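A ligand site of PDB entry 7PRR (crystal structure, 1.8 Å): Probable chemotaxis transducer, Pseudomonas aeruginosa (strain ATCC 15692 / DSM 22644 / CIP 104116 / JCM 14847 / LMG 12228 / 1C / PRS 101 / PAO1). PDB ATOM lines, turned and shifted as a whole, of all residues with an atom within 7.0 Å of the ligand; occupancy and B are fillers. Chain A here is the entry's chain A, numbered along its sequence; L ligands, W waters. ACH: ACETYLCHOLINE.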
ATOM      1  N   ASP A 111     -15.892 -11.968  25.104  1.00  0.00           N
ATOM      2  CA  ASP A 111     -15.253 -11.568  23.857  1.00  0.00           C
ATOM      3  C   ASP A 111     -15.840 -10.239  23.406  1.00  0.00           C
ATOM      4  O   ASP A 111     -16.653  -9.623  24.096  1.00  0.00           O
ATOM      5  CB  ASP A 111     -15.449 -12.657  22.780  1.00  0.00           C
ATOM      6  CG  ASP A 111     -16.906 -12.959  22.539  1.00  0.00           C
ATOM      7  OD1 ASP A 111     -17.756 -12.080  22.779  1.00  0.00           O
ATOM      8  OD2 ASP A 111     -17.234 -14.115  22.104  1.00  0.00           O
ATOM      9  N   THR A 112     -15.418  -9.814  22.214  1.00  0.00           N
ATOM     10  CA  THR A 112     -16.089  -8.764  21.450  1.00  0.00           C
ATOM     11  C   THR A 112     -15.820  -9.089  19.989  1.00  0.00           C
ATOM     12  O   THR A 112     -14.705  -9.512  19.653  1.00  0.00           O
ATOM     13  CB  THR A 112     -15.582  -7.352  21.808  1.00  0.00           C
ATOM     14  OG1 THR A 112     -15.807  -7.136  23.193  1.00  0.00           O
ATOM     15  CG2 THR A 112     -16.372  -6.288  21.071  1.00  0.00           C
ATOM     16  N   PHE A 113     -16.810  -8.899  19.141  1.00  0.00           N
ATOM     17  CA  PHE A 113     -16.623  -9.222  17.723  1.00  0.00           C
ATOM     18  C   PHE A 113     -17.425  -8.302  16.841  1.00  0.00           C
ATOM     19  O   PHE A 113     -18.401  -7.678  17.278  1.00  0.00           O
ATOM     20  CB  PHE A 113     -17.032 -10.669  17.482  1.00  0.00           C
ATOM     21  CG  PHE A 113     -18.424 -10.974  17.948  1.00  0.00           C
ATOM     22  CD1 PHE A 113     -18.645 -11.425  19.216  1.00  0.00           C
ATOM     23  CD2 PHE A 113     -19.483 -10.817  17.101  1.00  0.00           C
ATOM     24  CE1 PHE A 113     -19.910 -11.720  19.656  1.00  0.00           C
ATOM     25  CE2 PHE A 113     -20.754 -11.118  17.515  1.00  0.00           C
ATOM     26  CZ  PHE A 113     -20.963 -11.573  18.788  1.00  0.00           C
ATOM     27  N   LEU A 142     -13.998  -9.298   9.680  1.00  0.00           N
ATOM     28  CA  LEU A 142     -14.791 -10.231  10.478  1.00  0.00           C
ATOM     29  C   LEU A 142     -14.131 -10.633  11.788  1.00  0.00           C
ATOM     30  O   LEU A 142     -14.114 -11.823  12.155  1.00  0.00           O
ATOM     31  CB  LEU A 142     -15.063 -11.545   9.678  1.00  0.00           C
ATOM     32  CG  LEU A 142     -15.731 -11.466   8.314  1.00  0.00           C
ATOM     33  CD1 LEU A 142     -15.588 -12.811   7.574  1.00  0.00           C
ATOM     34  CD2 LEU A 142     -17.201 -11.096   8.510  1.00  0.00           C
ATOM     35  N   PRO A 143     -13.569  -9.688  12.539  1.00  0.00           N
ATOM     36  CA  PRO A 143     -12.784 -10.082  13.735  1.00  0.00           C
ATOM     37  C   PRO A 143     -13.612 -10.515  14.924  1.00  0.00           C
ATOM     38  O   PRO A 143     -14.612  -9.889  15.271  1.00  0.00           O
ATOM     39  CB  PRO A 143     -12.041  -8.781  14.112  1.00  0.00           C
ATOM     40  CG  PRO A 143     -13.000  -7.705  13.681  1.00  0.00           C
ATOM     41  CD  PRO A 143     -13.568  -8.222  12.355  1.00  0.00           C
ATOM     42  N   TRP A 144     -13.138 -11.574  15.574  1.00  0.00           N
ATOM     43  CA  TRP A 144     -13.633 -12.091  16.842  1.00  0.00           C
ATOM     44  C   TRP A 144     -12.471 -12.019  17.822  1.00  0.00           C
ATOM     45  O   TRP A 144     -11.511 -12.795  17.689  1.00  0.00           O
ATOM     46  CB  TRP A 144     -14.117 -13.523  16.639  1.00  0.00           C
ATOM     47  CG  TRP A 144     -14.644 -14.235  17.860  1.00  0.00           C
ATOM     48  CD1 TRP A 144     -15.089 -13.669  19.043  1.00  0.00           C
ATOM     49  CD2 TRP A 144     -14.808 -15.649  17.999  1.00  0.00           C
ATOM     50  NE1 TRP A 144     -15.516 -14.680  19.888  1.00  0.00           N
ATOM     51  CE2 TRP A 144     -15.342 -15.895  19.276  1.00  0.00           C
ATOM     52  CE3 TRP A 144     -14.537 -16.737  17.149  1.00  0.00           C
ATOM     53  CZ2 TRP A 144     -15.624 -17.175  19.735  1.00  0.00           C
ATOM     54  CZ3 TRP A 144     -14.808 -18.008  17.611  1.00  0.00           C
ATOM     55  CH2 TRP A 144     -15.349 -18.221  18.876  1.00  0.00           C
ATOM     56  N   GLU A 156      -9.589 -13.996  15.799  1.00  0.00           N
ATOM     57  CA  GLU A 156      -9.973 -15.040  14.855  1.00  0.00           C
ATOM     58  C   GLU A 156     -10.948 -14.439  13.854  1.00  0.00           C
ATOM     59  O   GLU A 156     -11.831 -13.672  14.230  1.00  0.00           O
ATOM     60  CB  GLU A 156     -10.629 -16.217  15.591  1.00  0.00           C
ATOM     61  CG  GLU A 156     -11.345 -17.240  14.701  1.00  0.00           C
ATOM     62  CD  GLU A 156     -11.748 -18.512  15.448  1.00  0.00           C
ATOM     63  OE1 GLU A 156     -11.280 -18.720  16.591  1.00  0.00           O
ATOM     64  OE2 GLU A 156     -12.496 -19.333  14.872  1.00  0.00           O
ATOM     65  N   ALA A 157     -10.796 -14.749  12.582  1.00  0.00           N
ATOM     66  CA  ALA A 157     -11.755 -14.243  11.598  1.00  0.00           C
ATOM     67  C   ALA A 157     -12.986 -15.167  11.623  1.00  0.00           C
ATOM     68  O   ALA A 157     -12.859 -16.393  11.688  1.00  0.00           O
ATOM     69  CB  ALA A 157     -11.143 -14.224  10.202  1.00  0.00           C
ATOM     70  N   MET A 158     -14.181 -14.600  11.569  1.00  0.00           N
ATOM     71  CA  MET A 158     -15.445 -15.357  11.619  1.00  0.00           C
ATOM     72  C   MET A 158     -15.906 -15.781  10.231  1.00  0.00           C
ATOM     73  O   MET A 158     -17.110 -15.940   9.987  1.00  0.00           O
ATOM     74  CB  MET A 158     -16.506 -14.476  12.274  1.00  0.00           C
ATOM     75  CG  MET A 158     -16.106 -13.736  13.533  1.00  0.00           C
ATOM     76  SD  MET A 158     -17.546 -13.181  14.538  1.00  0.00           S
ATOM     77  CE  MET A 158     -17.832 -11.677  13.812  1.00  0.00           C
ATOM     78  N   ALA A 159     -14.979 -16.033   9.308  1.00  0.00           N
ATOM     79  CA  ALA A 159     -15.351 -16.414   7.957  1.00  0.00           C
ATOM     80  C   ALA A 159     -16.123 -17.721   7.938  1.00  0.00           C
ATOM     81  O   ALA A 159     -17.005 -17.913   7.095  1.00  0.00           O
ATOM     82  CB  ALA A 159     -14.103 -16.540   7.084  1.00  0.00           C
ATOM     83  N   ASP A 160     -15.764 -18.638   8.838  1.00  0.00           N
ATOM     84  CA  ASP A 160     -16.351 -19.978   8.871  1.00  0.00           C
ATOM     85  C   ASP A 160     -17.803 -19.935   9.343  1.00  0.00           C
ATOM     86  O   ASP A 160     -18.649 -20.690   8.858  1.00  0.00           O
ATOM     87  CB  ASP A 160     -15.518 -20.901   9.791  1.00  0.00           C
ATOM     88  CG  ASP A 160     -15.439 -20.385  11.274  1.00  0.00           C
ATOM     89  OD1 ASP A 160     -15.382 -19.133  11.516  1.00  0.00           O
ATOM     90  OD2 ASP A 160     -15.380 -21.235  12.210  1.00  0.00           O
ATOM     91  N   SER A 161     -18.120 -19.049  10.284  1.00  0.00           N
ATOM     92  CA  SER A 161     -19.449 -19.050  10.884  1.00  0.00           C
ATOM     93  C   SER A 161     -20.391 -18.018  10.266  1.00  0.00           C
ATOM     94  O   SER A 161     -21.600 -18.242  10.282  1.00  0.00           O
ATOM     95  CB  SER A 161     -19.338 -18.821  12.400  1.00  0.00           C
ATOM     96  OG  SER A 161     -18.881 -17.503  12.724  1.00  0.00           O
ATOM     97  N   ILE A 162     -19.864 -16.964   9.655  1.00  0.00           N
ATOM     98  CA  ILE A 162     -20.698 -15.819   9.290  1.00  0.00           C
ATOM     99  C   ILE A 162     -21.737 -16.187   8.255  1.00  0.00           C
ATOM    100  O   ILE A 162     -22.826 -15.601   8.253  1.00  0.00           O
ATOM    101  CB  ILE A 162     -19.815 -14.639   8.818  1.00  0.00           C
ATOM    102  CG1 ILE A 162     -20.584 -13.320   8.927  1.00  0.00           C
ATOM    103  CG2 ILE A 162     -19.296 -14.817   7.420  1.00  0.00           C
ATOM    104  CD1 ILE A 162     -20.667 -12.781  10.318  1.00  0.00           C
ATOM    105  N   GLU A 174     -25.685 -21.506  13.180  1.00  0.00           N
ATOM    106  CA  GLU A 174     -24.359 -20.980  13.493  1.00  0.00           C
ATOM    107  C   GLU A 174     -24.217 -19.499  13.144  1.00  0.00           C
ATOM    108  O   GLU A 174     -23.454 -18.775  13.812  1.00  0.00           O
ATOM    109  CB  GLU A 174     -23.299 -21.790  12.748  1.00  0.00           C
ATOM    110  CG  GLU A 174     -21.882 -21.506  13.255  1.00  0.00           C
ATOM    111  CD  GLU A 174     -20.815 -22.430  12.682  1.00  0.00           C
ATOM    112  OE1 GLU A 174     -21.164 -23.317  11.859  1.00  0.00           O
ATOM    113  OE2 GLU A 174     -19.626 -22.238  13.042  1.00  0.00           O
ATOM    114  N   PHE A 177     -26.122 -14.960  14.937  1.00  0.00           N
ATOM    115  CA  PHE A 177     -25.622 -13.723  15.543  1.00  0.00           C
ATOM    116  C   PHE A 177     -25.556 -12.582  14.535  1.00  0.00           C
ATOM    117  O   PHE A 177     -25.617 -11.409  14.927  1.00  0.00           O
ATOM    118  CB  PHE A 177     -24.233 -13.941  16.196  1.00  0.00           C
ATOM    119  CG  PHE A 177     -23.143 -14.214  15.215  1.00  0.00           C
ATOM    120  CD1 PHE A 177     -22.946 -15.503  14.696  1.00  0.00           C
ATOM    121  CD2 PHE A 177     -22.282 -13.213  14.817  1.00  0.00           C
ATOM    122  CE1 PHE A 177     -21.928 -15.749  13.808  1.00  0.00           C
ATOM    123  CE2 PHE A 177     -21.274 -13.446  13.929  1.00  0.00           C
ATOM    124  CZ  PHE A 177     -21.103 -14.727  13.400  1.00  0.00           C
ATOM    125  N   PRO A 194     -23.131 -23.471  21.278  1.00  0.00           N
ATOM    126  CA  PRO A 194     -21.713 -23.814  21.445  1.00  0.00           C
ATOM    127  C   PRO A 194     -20.873 -23.338  20.281  1.00  0.00           C
ATOM    128  O   PRO A 194     -21.255 -23.469  19.116  1.00  0.00           O
ATOM    129  CB  PRO A 194     -21.727 -25.346  21.514  1.00  0.00           C
ATOM    130  CG  PRO A 194     -22.855 -25.720  20.569  1.00  0.00           C
ATOM    131  CD  PRO A 194     -23.896 -24.583  20.673  1.00  0.00           C
ATOM    132  N   TYR A 195     -19.706 -22.779  20.596  1.00  0.00           N
ATOM    133  CA  TYR A 195     -18.701 -22.436  19.599  1.00  0.00           C
ATOM    134  C   TYR A 195     -17.331 -22.899  20.079  1.00  0.00           C
ATOM    135  O   TYR A 195     -17.082 -22.956  21.288  1.00  0.00           O
ATOM    136  CB  TYR A 195     -18.676 -20.930  19.332  1.00  0.00           C
ATOM    137  CG  TYR A 195     -19.867 -20.415  18.574  1.00  0.00           C
ATOM    138  CD1 TYR A 195     -21.015 -19.987  19.253  1.00  0.00           C
ATOM    139  CD2 TYR A 195     -19.857 -20.342  17.172  1.00  0.00           C
ATOM    140  CE1 TYR A 195     -22.108 -19.476  18.546  1.00  0.00           C
ATOM    141  CE2 TYR A 195     -20.947 -19.828  16.479  1.00  0.00           C
ATOM    142  CZ  TYR A 195     -22.058 -19.422  17.168  1.00  0.00           C
ATOM    143  OH  TYR A 195     -23.152 -18.919  16.455  1.00  0.00           O
ATOM    144  N   GLU A 196     -16.482 -23.271  19.126  1.00  0.00           N
ATOM    145  CA  GLU A 196     -15.107 -23.632  19.434  1.00  0.00           C
ATOM    146  C   GLU A 196     -14.275 -22.398  19.722  1.00  0.00           C
ATOM    147  O   GLU A 196     -14.207 -21.495  18.891  1.00  0.00           O
ATOM    148  CB  GLU A 196     -14.473 -24.410  18.281  1.00  0.00           C
ATOM    149  CG  GLU A 196     -15.116 -25.712  17.932  1.00  0.00           C
ATOM    150  CD  GLU A 196     -15.130 -26.625  19.153  1.00  0.00           C
ATOM    151  OE1 GLU A 196     -14.154 -27.335  19.337  1.00  0.00           O
ATOM    152  OE2 GLU A 196     -16.147 -26.660  19.885  1.00  0.00           O
ATOM    153  N   MET A 197     -13.603 -22.391  20.866  1.00  0.00           N
ATOM    154  CA  MET A 197     -12.748 -21.271  21.269  1.00  0.00           C
ATOM    155  C   MET A 197     -11.445 -21.829  21.808  1.00  0.00           C
ATOM    156  O   MET A 197     -11.441 -22.486  22.857  1.00  0.00           O
ATOM    157  CB  MET A 197     -13.376 -20.416  22.360  1.00  0.00           C
ATOM    158  CG  MET A 197     -14.334 -19.418  21.938  1.00  0.00           C
ATOM    159  SD  MET A 197     -14.951 -18.558  23.419  1.00  0.00           S
ATOM    160  CE  MET A 197     -13.952 -17.076  23.389  1.00  0.00           C
ATOM    161  N   MET A 204     -22.483 -20.296  24.968  1.00  0.00           N
ATOM    162  CA  MET A 204     -22.560 -18.829  25.152  1.00  0.00           C
ATOM    163  C   MET A 204     -23.790 -18.217  24.523  1.00  0.00           C
ATOM    164  O   MET A 204     -24.457 -18.832  23.719  1.00  0.00           O
ATOM    165  CB  MET A 204     -21.280 -18.169  24.576  1.00  0.00           C
ATOM    166  CG  MET A 204     -21.311 -18.140  23.045  1.00  0.00           C
ATOM    167  SD  MET A 204     -19.706 -17.769  22.312  1.00  0.00           S
ATOM    168  CE  MET A 204     -18.695 -19.106  22.787  1.00  0.00           C
ATOM    169  N   SER A 205     -24.145 -17.028  24.991  1.00  0.00           N
ATOM    170  CA  SER A 205     -25.215 -16.251  24.407  1.00  0.00           C
ATOM    171  C   SER A 205     -24.612 -14.954  23.911  1.00  0.00           C
ATOM    172  O   SER A 205     -23.769 -14.361  24.588  1.00  0.00           O
ATOM    173  CB  SER A 205     -26.357 -15.995  25.382  1.00  0.00           C
ATOM    174  OG  SER A 205     -27.356 -17.016  25.260  1.00  0.00           O
ATOM    175  N   SER A 206     -25.036 -14.514  22.721  1.00  0.00           N
ATOM    176  CA  SER A 206     -24.456 -13.339  22.086  1.00  0.00           C
ATOM    177  C   SER A 206     -25.448 -12.188  22.145  1.00  0.00           C
ATOM    178  O   SER A 206     -26.665 -12.386  22.069  1.00  0.00           O
ATOM    179  CB  SER A 206     -24.039 -13.580  20.630  1.00  0.00           C
ATOM    180  OG  SER A 206     -25.157 -13.922  19.854  1.00  0.00           O
ATOM    181  N   ASN A 208     -26.063  -8.630  20.302  1.00  0.00           N
ATOM    182  CA  ASN A 208     -25.704  -8.121  18.988  1.00  0.00           C
ATOM    183  C   ASN A 208     -26.510  -6.878  18.617  1.00  0.00           C
ATOM    184  O   ASN A 208     -27.697  -6.829  18.874  1.00  0.00           O
ATOM    185  CB  ASN A 208     -25.989  -9.214  17.926  1.00  0.00           C
ATOM    186  CG  ASN A 208     -25.346 -10.514  18.289  1.00  0.00           C
ATOM    187  OD1 ASN A 208     -24.164 -10.671  18.161  1.00  0.00           O
ATOM    188  ND2 ASN A 208     -26.133 -11.439  18.839  1.00  0.00           N
ATOM    189  N   GLY A 222     -21.030  -7.376  18.361  1.00  0.00           N
ATOM    190  CA  GLY A 222     -21.591  -8.182  19.417  1.00  0.00           C
ATOM    191  C   GLY A 222     -20.570  -8.520  20.469  1.00  0.00           C
ATOM    192  O   GLY A 222     -19.366  -8.300  20.313  1.00  0.00           O
ATOM    193  N   ALA A 223     -21.098  -9.019  21.584  1.00  0.00           N
ATOM    194  CA  ALA A 223     -20.264  -9.626  22.643  1.00  0.00           C
ATOM    195  C   ALA A 223     -21.024 -10.803  23.225  1.00  0.00           C
ATOM    196  O   ALA A 223     -22.246 -10.786  23.335  1.00  0.00           O
ATOM    197  CB  ALA A 223     -19.889  -8.615  23.730  1.00  0.00           C
ATOM    198  N   ASP A 224     -20.285 -11.817  23.637  1.00  0.00           N
ATOM    199  CA  ASP A 224     -20.887 -12.996  24.264  1.00  0.00           C
ATOM    200  C   ASP A 224     -20.732 -12.917  25.801  1.00  0.00           C
ATOM    201  O   ASP A 224     -19.746 -12.379  26.328  1.00  0.00           O
ATOM    202  CB  ASP A 224     -20.172 -14.251  23.752  1.00  0.00           C
ATOM    203  CG  ASP A 224     -20.423 -14.540  22.269  1.00  0.00           C
ATOM    204  OD1 ASP A 224     -21.573 -14.759  21.891  1.00  0.00           O
ATOM    205  OD2 ASP A 224     -19.470 -14.525  21.482  1.00  0.00           O
HETATM  206  N1  ACH L   1     -19.529 -15.780  17.826  1.00  0.00           N
HETATM  207  C2  ACH L   1     -19.675 -16.098  16.451  1.00  0.00           C
HETATM  208  C3  ACH L   1     -18.372 -16.389  15.749  1.00  0.00           C
HETATM  209  O4  ACH L   1     -18.063 -17.739  15.930  1.00  0.00           O
HETATM  210  C5  ACH L   1     -17.056 -18.249  15.081  1.00  0.00           C
HETATM  211  O7  ACH L   1     -16.518 -17.532  14.288  1.00  0.00           O
HETATM  212  C6  ACH L   1     -16.657 -19.720  15.199  1.00  0.00           C
HETATM  213  C8  ACH L   1     -20.890 -15.431  18.336  1.00  0.00           C
HETATM  214  C9  ACH L   1     -19.000 -16.860  18.631  1.00  0.00           C
HETATM  215  C10 ACH L   1     -18.635 -14.613  18.046  1.00  0.00           C
HETATM  216  O   HOH W   1     -13.942 -21.427  16.037  1.00  0.00           O
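The backbone NH (N) of Trp 144 sits at hydrogen-bond distance from the backbone carbonyl oxygen (O) of Glu 156 (2.8 Å).
OD2 of Asp 111 is in hydrogen-bond range of NE1 of Trp 144 (2.9 Å).
N of Gly 222 is in hydrogen-bond range of O of Phe 113.
The side-chain hydroxyl (OH) of Tyr 195 is in hydrogen-bond range of the backbone carbonyl oxygen (O) of Glu 174, at 2.7 Å.
The backbone carbonyl oxygen (O) of Leu 142 lies within hydrogen-bond range of the backbone NH (N) of Met 158, at 2.8 Å.
The side-chain carboxylate (OD1) of Asp 111 sits at hydrogen-bond distance from the backbone NH (N) of Asp 224 (2.7 Å).
O7 of the ligand lies within hydrogen-bond range of OG of Ser 161 (2.8 Å).
N1 of the ligand lies within salt-bridge range of OD2 of Asp 224, at 3.9 Å.
An oxygen (O7) of the ligand lies close to the side-chain carboxylate of Asp 160 (3.4 Å).
Phe 113 touches the ligand (CD1 to C10, 3.4 Å).
Trp 144 touches the ligand (CZ3 to C5, 3.4 Å).
Met 158 touches the ligand (SD to C3, 3.5 Å).
Phe 177 touches the ligand (CE1 to C2, 3.5 Å).
Tyr 195 touches the ligand (CD2 to O4, 3.4 Å).
Met 204 touches the ligand.
Hydrophobic or aromatic side chains within 4 Å of the ligand: Phe 113, Trp 144, Met 158, Phe 177, Tyr 195 and Met 204.
Of the 26 residues printed, 9 come within 4 Å of the ligand.
Water W1 lies within hydrogen-bond range of OE2 of Glu 156 and O of Glu 196.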
